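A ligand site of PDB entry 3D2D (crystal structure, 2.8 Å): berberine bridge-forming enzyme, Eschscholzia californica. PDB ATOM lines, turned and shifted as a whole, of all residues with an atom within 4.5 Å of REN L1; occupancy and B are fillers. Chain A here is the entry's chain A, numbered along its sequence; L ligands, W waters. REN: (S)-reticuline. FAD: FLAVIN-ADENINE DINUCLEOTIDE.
Water W1 lies within hydrogen-bond range of ND2 of Asn 390 (2.8 Å), O of Ala 388 (3.4 Å) and O20 of REN L1 (3.4 Å).
Residues that only touch REN L1: Tyr 106 (3.2 Å), Trp 165 (3.2 Å), Ser 280 (3.97 Å), Leu 282 (3.4 Å), Leu 295 (3.6 Å), Arg 354 (3.5 Å), Phe 356 (3.5 Å), Phe 386 (3.8 Å), Ala 388 (3.4 Å) and Ala 421 (3.5 Å).
Hydrophobic or aromatic side chains within 4 Å of REN L1: Tyr 106, Trp 165, Leu 282, Leu 295, Phe 356, Phe 386, Ala 388 and Ala 421.
13 residues have an atom within 4 Å of REN L1: Tyr 106, Trp 165, Ser 280, Leu 282, Leu 295, Asp 352, Arg 354, Phe 356, Phe 386, Ala 388, Asn 390, Glu 417 and Ala 421.
OD1 of Asp 352 sits at hydrogen-bond distance from O4 of REN L1.
An oxygen (O20) of REN L1 is in hydrogen-bond range of the side-chain carboxylate (OE1) of Glu 417, 2.8 Å away.
O20 of REN L1 lies within hydrogen-bond range of ND2 of Asn 390.
The side-chain sulfur (SG) of Cys 166 is covalently linked to a carbon (C6) of FAD L2, 1.8 Å away.
The side-chain carboxylate (OD2) of Asp 352 is in salt-bridge range of the guanidinium group (NH2) of Arg 354 (2.7 Å).
O of Glu 417 sits at hydrogen-bond distance from N of Ala 388, 2.7 Å away.
The side-chain amide oxygen of Asn 390 is in hydrogen-bond range of the side-chain hydroxyl of Ser 280.
The guanidinium group (NH1) of Arg 354 lies within hydrogen-bond range of the backbone carbonyl oxygen (O) of Ala 421 (3.4 Å).
The backbone carbonyl oxygen of Leu 295 sits at hydrogen-bond distance from the backbone NH of Ser 280 (2.8 Å).
The backbone carbonyl oxygen (O) of Phe 386 lies within hydrogen-bond range of the backbone NH (N) of Ile 419, at 2.9 Å.
SD of Met 182 is in hydrogen-bond range of OG of Ser 280 (3.5 Å).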
ATOM      1  N   TYR A 106     -22.922 -13.582   6.296  1.00  0.00           N
ATOM      2  CA  TYR A 106     -22.810 -14.903   6.899  1.00  0.00           C
ATOM      3  C   TYR A 106     -23.819 -15.079   8.034  1.00  0.00           C
ATOM      4  O   TYR A 106     -24.146 -16.205   8.408  1.00  0.00           O
ATOM      5  CB  TYR A 106     -21.391 -15.170   7.412  1.00  0.00           C
ATOM      6  CG  TYR A 106     -20.363 -15.337   6.327  1.00  0.00           C
ATOM      7  CD1 TYR A 106     -20.717 -15.824   5.071  1.00  0.00           C
ATOM      8  CD2 TYR A 106     -19.020 -15.036   6.546  1.00  0.00           C
ATOM      9  CE1 TYR A 106     -19.777 -15.984   4.081  1.00  0.00           C
ATOM     10  CE2 TYR A 106     -18.066 -15.196   5.560  1.00  0.00           C
ATOM     11  CZ  TYR A 106     -18.454 -15.672   4.322  1.00  0.00           C
ATOM     12  OH  TYR A 106     -17.514 -15.832   3.332  1.00  0.00           O
ATOM     13  N   TRP A 165     -14.093 -13.411  -4.717  1.00  0.00           N
ATOM     14  CA  TRP A 165     -14.256 -14.266  -5.876  1.00  0.00           C
ATOM     15  C   TRP A 165     -15.727 -14.564  -6.137  1.00  0.00           C
ATOM     16  O   TRP A 165     -16.092 -14.978  -7.237  1.00  0.00           O
ATOM     17  CB  TRP A 165     -13.459 -15.559  -5.709  1.00  0.00           C
ATOM     18  CG  TRP A 165     -13.922 -16.401  -4.556  1.00  0.00           C
ATOM     19  CD1 TRP A 165     -13.419 -16.384  -3.285  1.00  0.00           C
ATOM     20  CD2 TRP A 165     -14.974 -17.371  -4.571  1.00  0.00           C
ATOM     21  NE1 TRP A 165     -14.104 -17.291  -2.503  1.00  0.00           N
ATOM     22  CE2 TRP A 165     -15.058 -17.913  -3.274  1.00  0.00           C
ATOM     23  CE3 TRP A 165     -15.860 -17.832  -5.555  1.00  0.00           C
ATOM     24  CZ2 TRP A 165     -15.992 -18.893  -2.931  1.00  0.00           C
ATOM     25  CZ3 TRP A 165     -16.780 -18.811  -5.209  1.00  0.00           C
ATOM     26  CH2 TRP A 165     -16.835 -19.334  -3.914  1.00  0.00           C
ATOM     27  N   CYS A 166     -16.570 -14.341  -5.136  1.00  0.00           N
ATOM     28  CA  CYS A 166     -18.003 -14.619  -5.252  1.00  0.00           C
ATOM     29  C   CYS A 166     -18.732 -13.558  -6.072  1.00  0.00           C
ATOM     30  O   CYS A 166     -18.954 -12.442  -5.612  1.00  0.00           O
ATOM     31  CB  CYS A 166     -18.639 -14.738  -3.857  1.00  0.00           C
ATOM     32  SG  CYS A 166     -17.984 -16.106  -2.876  1.00  0.00           S
ATOM     33  N   MET A 182      -8.484 -12.507  -4.798  1.00  0.00           N
ATOM     34  CA  MET A 182      -7.291 -13.140  -5.358  1.00  0.00           C
ATOM     35  C   MET A 182      -6.238 -12.130  -5.806  1.00  0.00           C
ATOM     36  O   MET A 182      -5.101 -12.496  -6.106  1.00  0.00           O
ATOM     37  CB  MET A 182      -7.659 -14.034  -6.541  1.00  0.00           C
ATOM     38  CG  MET A 182      -8.427 -15.287  -6.161  1.00  0.00           C
ATOM     39  SD  MET A 182      -7.418 -16.498  -5.279  1.00  0.00           S
ATOM     40  CE  MET A 182      -6.307 -17.035  -6.575  1.00  0.00           C
ATOM     41  N   SER A 280      -4.084 -19.934  -3.326  1.00  0.00           N
ATOM     42  CA  SER A 280      -5.033 -20.187  -2.252  1.00  0.00           C
ATOM     43  C   SER A 280      -5.404 -21.669  -2.224  1.00  0.00           C
ATOM     44  O   SER A 280      -5.253 -22.367  -3.226  1.00  0.00           O
ATOM     45  CB  SER A 280      -6.273 -19.317  -2.431  1.00  0.00           C
ATOM     46  OG  SER A 280      -5.912 -17.950  -2.494  1.00  0.00           O
ATOM     47  N   LEU A 282      -8.234 -24.822  -0.874  1.00  0.00           N
ATOM     48  CA  LEU A 282      -9.510 -25.271  -0.352  1.00  0.00           C
ATOM     49  C   LEU A 282      -9.357 -26.712   0.095  1.00  0.00           C
ATOM     50  O   LEU A 282      -9.274 -27.628  -0.722  1.00  0.00           O
ATOM     51  CB  LEU A 282     -10.592 -25.165  -1.435  1.00  0.00           C
ATOM     52  CG  LEU A 282     -11.093 -23.759  -1.759  1.00  0.00           C
ATOM     53  CD1 LEU A 282     -11.838 -23.738  -3.086  1.00  0.00           C
ATOM     54  CD2 LEU A 282     -11.980 -23.265  -0.635  1.00  0.00           C
ATOM     55  N   LEU A 295      -5.959 -23.090  -5.843  1.00  0.00           N
ATOM     56  CA  LEU A 295      -6.423 -21.991  -6.678  1.00  0.00           C
ATOM     57  C   LEU A 295      -5.274 -21.035  -6.914  1.00  0.00           C
ATOM     58  O   LEU A 295      -4.822 -20.339  -6.000  1.00  0.00           O
ATOM     59  CB  LEU A 295      -7.581 -21.262  -6.002  1.00  0.00           C
ATOM     60  CG  LEU A 295      -8.824 -22.088  -5.692  1.00  0.00           C
ATOM     61  CD1 LEU A 295      -9.901 -21.213  -5.067  1.00  0.00           C
ATOM     62  CD2 LEU A 295      -9.333 -22.751  -6.950  1.00  0.00           C
ATOM     63  N   ASP A 352     -23.877 -22.521  -4.291  1.00  0.00           N
ATOM     64  CA  ASP A 352     -23.944 -23.802  -3.584  1.00  0.00           C
ATOM     65  C   ASP A 352     -25.376 -24.250  -3.351  1.00  0.00           C
ATOM     66  O   ASP A 352     -25.710 -25.421  -3.577  1.00  0.00           O
ATOM     67  CB  ASP A 352     -23.197 -23.729  -2.245  1.00  0.00           C
ATOM     68  CG  ASP A 352     -21.973 -24.630  -2.208  1.00  0.00           C
ATOM     69  OD1 ASP A 352     -21.218 -24.666  -3.200  1.00  0.00           O
ATOM     70  OD2 ASP A 352     -21.777 -25.310  -1.184  1.00  0.00           O
ATOM     71  N   ARG A 354     -26.476 -24.411  -0.530  1.00  0.00           N
ATOM     72  CA  ARG A 354     -26.364 -25.061   0.781  1.00  0.00           C
ATOM     73  C   ARG A 354     -26.244 -24.057   1.920  1.00  0.00           C
ATOM     74  O   ARG A 354     -25.542 -23.058   1.816  1.00  0.00           O
ATOM     75  CB  ARG A 354     -25.153 -26.005   0.819  1.00  0.00           C
ATOM     76  CG  ARG A 354     -25.316 -27.302   0.044  1.00  0.00           C
ATOM     77  CD  ARG A 354     -24.129 -28.209   0.300  1.00  0.00           C
ATOM     78  NE  ARG A 354     -22.856 -27.526   0.067  1.00  0.00           N
ATOM     79  CZ  ARG A 354     -21.675 -27.953   0.500  1.00  0.00           C
ATOM     80  NH1 ARG A 354     -21.591 -29.076   1.194  1.00  0.00           N
ATOM     81  NH2 ARG A 354     -20.577 -27.249   0.236  1.00  0.00           N
ATOM     82  N   ALA A 355     -26.942 -24.342   3.018  1.00  0.00           N
ATOM     83  CA  ALA A 355     -26.791 -23.547   4.234  1.00  0.00           C
ATOM     84  C   ALA A 355     -25.378 -23.726   4.767  1.00  0.00           C
ATOM     85  O   ALA A 355     -24.720 -24.714   4.446  1.00  0.00           O
ATOM     86  CB  ALA A 355     -27.822 -23.962   5.278  1.00  0.00           C
ATOM     87  N   PHE A 356     -24.901 -22.783   5.576  1.00  0.00           N
ATOM     88  CA  PHE A 356     -23.536 -22.848   6.082  1.00  0.00           C
ATOM     89  C   PHE A 356     -23.288 -21.879   7.239  1.00  0.00           C
ATOM     90  O   PHE A 356     -24.005 -20.900   7.413  1.00  0.00           O
ATOM     91  CB  PHE A 356     -22.541 -22.555   4.960  1.00  0.00           C
ATOM     92  CG  PHE A 356     -22.536 -21.122   4.524  1.00  0.00           C
ATOM     93  CD1 PHE A 356     -21.683 -20.205   5.103  1.00  0.00           C
ATOM     94  CD2 PHE A 356     -23.384 -20.679   3.515  1.00  0.00           C
ATOM     95  CE1 PHE A 356     -21.669 -18.877   4.705  1.00  0.00           C
ATOM     96  CE2 PHE A 356     -23.381 -19.357   3.101  1.00  0.00           C
ATOM     97  CZ  PHE A 356     -22.524 -18.456   3.696  1.00  0.00           C
ATOM     98  N   THR A 358     -19.641 -20.133   8.841  1.00  0.00           N
ATOM     99  CA  THR A 358     -18.195 -20.031   8.650  1.00  0.00           C
ATOM    100  C   THR A 358     -17.518 -19.169   9.701  1.00  0.00           C
ATOM    101  O   THR A 358     -17.940 -18.042   9.959  1.00  0.00           O
ATOM    102  CB  THR A 358     -17.832 -19.516   7.227  1.00  0.00           C
ATOM    103  OG1 THR A 358     -16.461 -19.104   7.190  1.00  0.00           O
ATOM    104  CG2 THR A 358     -18.704 -18.332   6.836  1.00  0.00           C
ATOM    105  N   PHE A 386     -14.966 -27.907   5.465  1.00  0.00           N
ATOM    106  CA  PHE A 386     -13.805 -27.650   4.628  1.00  0.00           C
ATOM    107  C   PHE A 386     -13.158 -26.330   5.015  1.00  0.00           C
ATOM    108  O   PHE A 386     -13.823 -25.411   5.497  1.00  0.00           O
ATOM    109  CB  PHE A 386     -14.174 -27.692   3.136  1.00  0.00           C
ATOM    110  CG  PHE A 386     -15.127 -26.610   2.701  1.00  0.00           C
ATOM    111  CD1 PHE A 386     -14.658 -25.381   2.265  1.00  0.00           C
ATOM    112  CD2 PHE A 386     -16.493 -26.832   2.720  1.00  0.00           C
ATOM    113  CE1 PHE A 386     -15.533 -24.394   1.855  1.00  0.00           C
ATOM    114  CE2 PHE A 386     -17.377 -25.841   2.315  1.00  0.00           C
ATOM    115  CZ  PHE A 386     -16.895 -24.621   1.887  1.00  0.00           C
ATOM    116  N   ALA A 388     -10.596 -22.950   4.059  1.00  0.00           N
ATOM    117  CA  ALA A 388     -10.125 -22.080   2.991  1.00  0.00           C
ATOM    118  C   ALA A 388      -8.891 -21.353   3.492  1.00  0.00           C
ATOM    119  O   ALA A 388      -8.946 -20.634   4.484  1.00  0.00           O
ATOM    120  CB  ALA A 388     -11.203 -21.098   2.605  1.00  0.00           C
ATOM    121  N   ASN A 390      -5.924 -18.636   2.775  1.00  0.00           N
ATOM    122  CA  ASN A 390      -5.468 -17.505   1.980  1.00  0.00           C
ATOM    123  C   ASN A 390      -4.220 -16.846   2.550  1.00  0.00           C
ATOM    124  O   ASN A 390      -4.108 -16.659   3.760  1.00  0.00           O
ATOM    125  CB  ASN A 390      -6.581 -16.469   1.825  1.00  0.00           C
ATOM    126  CG  ASN A 390      -7.519 -16.790   0.679  1.00  0.00           C
ATOM    127  OD1 ASN A 390      -7.095 -16.841  -0.478  1.00  0.00           O
ATOM    128  ND2 ASN A 390      -8.787 -17.007   0.987  1.00  0.00           N
ATOM    129  N   GLU A 417      -9.880 -20.109   7.168  1.00  0.00           N
ATOM    130  CA  GLU A 417     -11.336 -19.983   7.157  1.00  0.00           C
ATOM    131  C   GLU A 417     -11.976 -21.364   7.261  1.00  0.00           C
ATOM    132  O   GLU A 417     -11.744 -22.233   6.427  1.00  0.00           O
ATOM    133  CB  GLU A 417     -11.769 -19.272   5.873  1.00  0.00           C
ATOM    134  CG  GLU A 417     -13.244 -18.912   5.792  1.00  0.00           C
ATOM    135  CD  GLU A 417     -13.583 -18.074   4.559  1.00  0.00           C
ATOM    136  OE1 GLU A 417     -12.642 -17.593   3.880  1.00  0.00           O
ATOM    137  OE2 GLU A 417     -14.783 -17.900   4.292  1.00  0.00           O
ATOM    138  N   ILE A 419     -15.307 -23.654   7.260  1.00  0.00           N
ATOM    139  CA  ILE A 419     -16.691 -23.637   6.812  1.00  0.00           C
ATOM    140  C   ILE A 419     -17.350 -24.975   7.052  1.00  0.00           C
ATOM    141  O   ILE A 419     -16.687 -26.006   7.139  1.00  0.00           O
ATOM    142  CB  ILE A 419     -16.793 -23.286   5.311  1.00  0.00           C
ATOM    143  CG1 ILE A 419     -15.975 -22.028   4.998  1.00  0.00           C
ATOM    144  CG2 ILE A 419     -18.257 -23.111   4.904  1.00  0.00           C
ATOM    145  CD1 ILE A 419     -14.523 -22.291   4.736  1.00  0.00           C
ATOM    146  N   ALA A 421     -21.095 -26.745   5.525  1.00  0.00           N
ATOM    147  CA  ALA A 421     -22.296 -26.531   4.747  1.00  0.00           C
ATOM    148  C   ALA A 421     -23.046 -27.840   4.603  1.00  0.00           C
ATOM    149  O   ALA A 421     -22.442 -28.904   4.514  1.00  0.00           O
ATOM    150  CB  ALA A 421     -21.948 -25.968   3.378  1.00  0.00           C
HETATM  151  C2  REN L   1     -17.971 -21.725  -0.618  1.00  0.00           C
HETATM  152  C3  REN L   1     -19.019 -22.628  -0.535  1.00  0.00           C
HETATM  153  C5  REN L   1     -19.916 -22.560   0.526  1.00  0.00           C
HETATM  154  C8  REN L   1     -19.762 -21.580   1.500  1.00  0.00           C
HETATM  155  C9  REN L   1     -18.714 -20.677   1.417  1.00  0.00           C
HETATM  156  C10 REN L   1     -18.427 -19.803   2.638  1.00  0.00           C
HETATM  157  C11 REN L   1     -17.244 -18.867   2.412  1.00  0.00           C
HETATM  158  N12 REN L   1     -17.115 -18.596   0.992  1.00  0.00           N
HETATM  159  C14 REN L   1     -16.696 -19.795   0.268  1.00  0.00           C
HETATM  160  C16 REN L   1     -15.464 -20.463   0.880  1.00  0.00           C
HETATM  161  C17 REN L   1     -14.147 -19.911   0.326  1.00  0.00           C
HETATM  162  C25 REN L   1     -13.677 -20.327  -0.917  1.00  0.00           C
HETATM  163  C24 REN L   1     -12.482 -19.814  -1.410  1.00  0.00           C
HETATM  164  C21 REN L   1     -11.750 -18.897  -0.661  1.00  0.00           C
HETATM  165  O22 REN L   1     -10.565 -18.400  -1.142  1.00  0.00           O
HETATM  166  C23 REN L   1     -10.188 -18.653  -2.504  1.00  0.00           C
HETATM  167  C19 REN L   1     -12.220 -18.491   0.586  1.00  0.00           C
HETATM  168  O20 REN L   1     -11.525 -17.590   1.341  1.00  0.00           O
HETATM  169  C18 REN L   1     -13.420 -19.007   1.072  1.00  0.00           C
HETATM  170  C1  REN L   1     -17.818 -20.745   0.356  1.00  0.00           C
HETATM  171  C13 REN L   1     -16.247 -17.451   0.754  1.00  0.00           C
HETATM  172  O6  REN L   1     -20.949 -23.445   0.604  1.00  0.00           O
HETATM  173  C7  REN L   1     -22.120 -23.081   1.348  1.00  0.00           C
HETATM  174  O4  REN L   1     -19.183 -23.591  -1.497  1.00  0.00           O
HETATM  175  PA  FAD L   2     -25.525  -8.211   2.399  1.00  0.00           P
HETATM  176  O1A FAD L   2     -26.221  -9.173   3.324  1.00  0.00           O
HETATM  177  O2A FAD L   2     -26.476  -7.642   1.382  1.00  0.00           O
HETATM  178  O5B FAD L   2     -24.878  -7.016   3.257  1.00  0.00           O
HETATM  179  C5B FAD L   2     -23.944  -7.293   4.280  1.00  0.00           C
HETATM  180  C4B FAD L   2     -24.039  -6.198   5.338  1.00  0.00           C
HETATM  181  O4B FAD L   2     -23.804  -4.931   4.751  1.00  0.00           O
HETATM  182  C3B FAD L   2     -25.415  -6.166   5.949  1.00  0.00           C
HETATM  183  O3B FAD L   2     -25.302  -5.882   7.322  1.00  0.00           O
HETATM  184  C2B FAD L   2     -26.091  -4.991   5.289  1.00  0.00           C
HETATM  185  O2B FAD L   2     -26.958  -4.358   6.189  1.00  0.00           O
HETATM  186  C1B FAD L   2     -24.929  -4.089   4.913  1.00  0.00           C
HETATM  187  N9A FAD L   2     -25.205  -3.394   3.644  1.00  0.00           N
HETATM  188  C8A FAD L   2     -25.723  -3.957   2.504  1.00  0.00           C
HETATM  189  N7A FAD L   2     -25.833  -2.988   1.572  1.00  0.00           N
HETATM  190  C5A FAD L   2     -25.394  -1.833   2.091  1.00  0.00           C
HETATM  191  C6A FAD L   2     -25.303  -0.551   1.558  1.00  0.00           C
HETATM  192  N6A FAD L   2     -25.436  -0.377   0.239  1.00  0.00           N
HETATM  193  N1A FAD L   2     -24.805   0.474   2.332  1.00  0.00           N
HETATM  194  C2A FAD L   2     -24.411   0.226   3.631  1.00  0.00           C
HETATM  195  N3A FAD L   2     -24.507  -1.050   4.153  1.00  0.00           N
HETATM  196  C4A FAD L   2     -24.993  -2.059   3.390  1.00  0.00           C
HETATM  197  N1  FAD L   2     -16.056 -12.267   1.886  1.00  0.00           N
HETATM  198  C2  FAD L   2     -14.760 -11.914   1.568  1.00  0.00           C
HETATM  199  O2  FAD L   2     -14.236 -10.940   2.116  1.00  0.00           O
HETATM  200  N3  FAD L   2     -14.100 -12.549   0.528  1.00  0.00           N
HETATM  201  C4  FAD L   2     -14.755 -13.500  -0.209  1.00  0.00           C
HETATM  202  O4  FAD L   2     -14.177 -14.023  -1.163  1.00  0.00           O
HETATM  203  C4X FAD L   2     -16.064 -13.854   0.106  1.00  0.00           C
HETATM  204  N5  FAD L   2     -16.732 -14.778  -0.671  1.00  0.00           N
HETATM  205  C5X FAD L   2     -18.082 -14.995  -0.473  1.00  0.00           C
HETATM  206  C6  FAD L   2     -18.764 -15.851  -1.319  1.00  0.00           C
HETATM  207  C7  FAD L   2     -20.131 -16.059  -1.177  1.00  0.00           C
HETATM  208  C7M FAD L   2     -20.838 -17.049  -2.054  1.00  0.00           C
HETATM  209  C8  FAD L   2     -20.813 -15.430  -0.132  1.00  0.00           C
HETATM  210  C8M FAD L   2     -22.306 -15.603   0.017  1.00  0.00           C
HETATM  211  C9  FAD L   2     -20.125 -14.563   0.718  1.00  0.00           C
HETATM  212  C9A FAD L   2     -18.759 -14.336   0.543  1.00  0.00           C
HETATM  213  N10 FAD L   2     -18.063 -13.480   1.393  1.00  0.00           N
HETATM  214  C10 FAD L   2     -16.724 -13.218   1.146  1.00  0.00           C
HETATM  215  C1' FAD L   2     -18.789 -12.710   2.448  1.00  0.00           C
HETATM  216  C2' FAD L   2     -19.086 -11.294   1.969  1.00  0.00           C
HETATM  217  O2' FAD L   2     -17.887 -10.553   1.825  1.00  0.00           O
HETATM  218  C3' FAD L   2     -19.975 -10.545   2.952  1.00  0.00           C
HETATM  219  O3' FAD L   2     -21.201 -11.235   3.081  1.00  0.00           O
HETATM  220  C4' FAD L   2     -20.260  -9.152   2.424  1.00  0.00           C
HETATM  221  O4' FAD L   2     -21.025  -8.448   3.379  1.00  0.00           O
HETATM  222  C5' FAD L   2     -21.019  -9.234   1.110  1.00  0.00           C
HETATM  223  O5' FAD L   2     -21.970  -8.196   1.036  1.00  0.00           O
HETATM  224  P   FAD L   2     -23.431  -8.511   0.431  1.00  0.00           P
HETATM  225  O1P FAD L   2     -24.007  -7.263  -0.198  1.00  0.00           O
HETATM  226  O2P FAD L   2     -23.352  -9.618  -0.584  1.00  0.00           O
HETATM  227  O3P FAD L   2     -24.274  -8.989   1.730  1.00  0.00           O
HETATM  228  O   HOH W   1      -9.100 -17.379   3.706  1.00  0.00           O
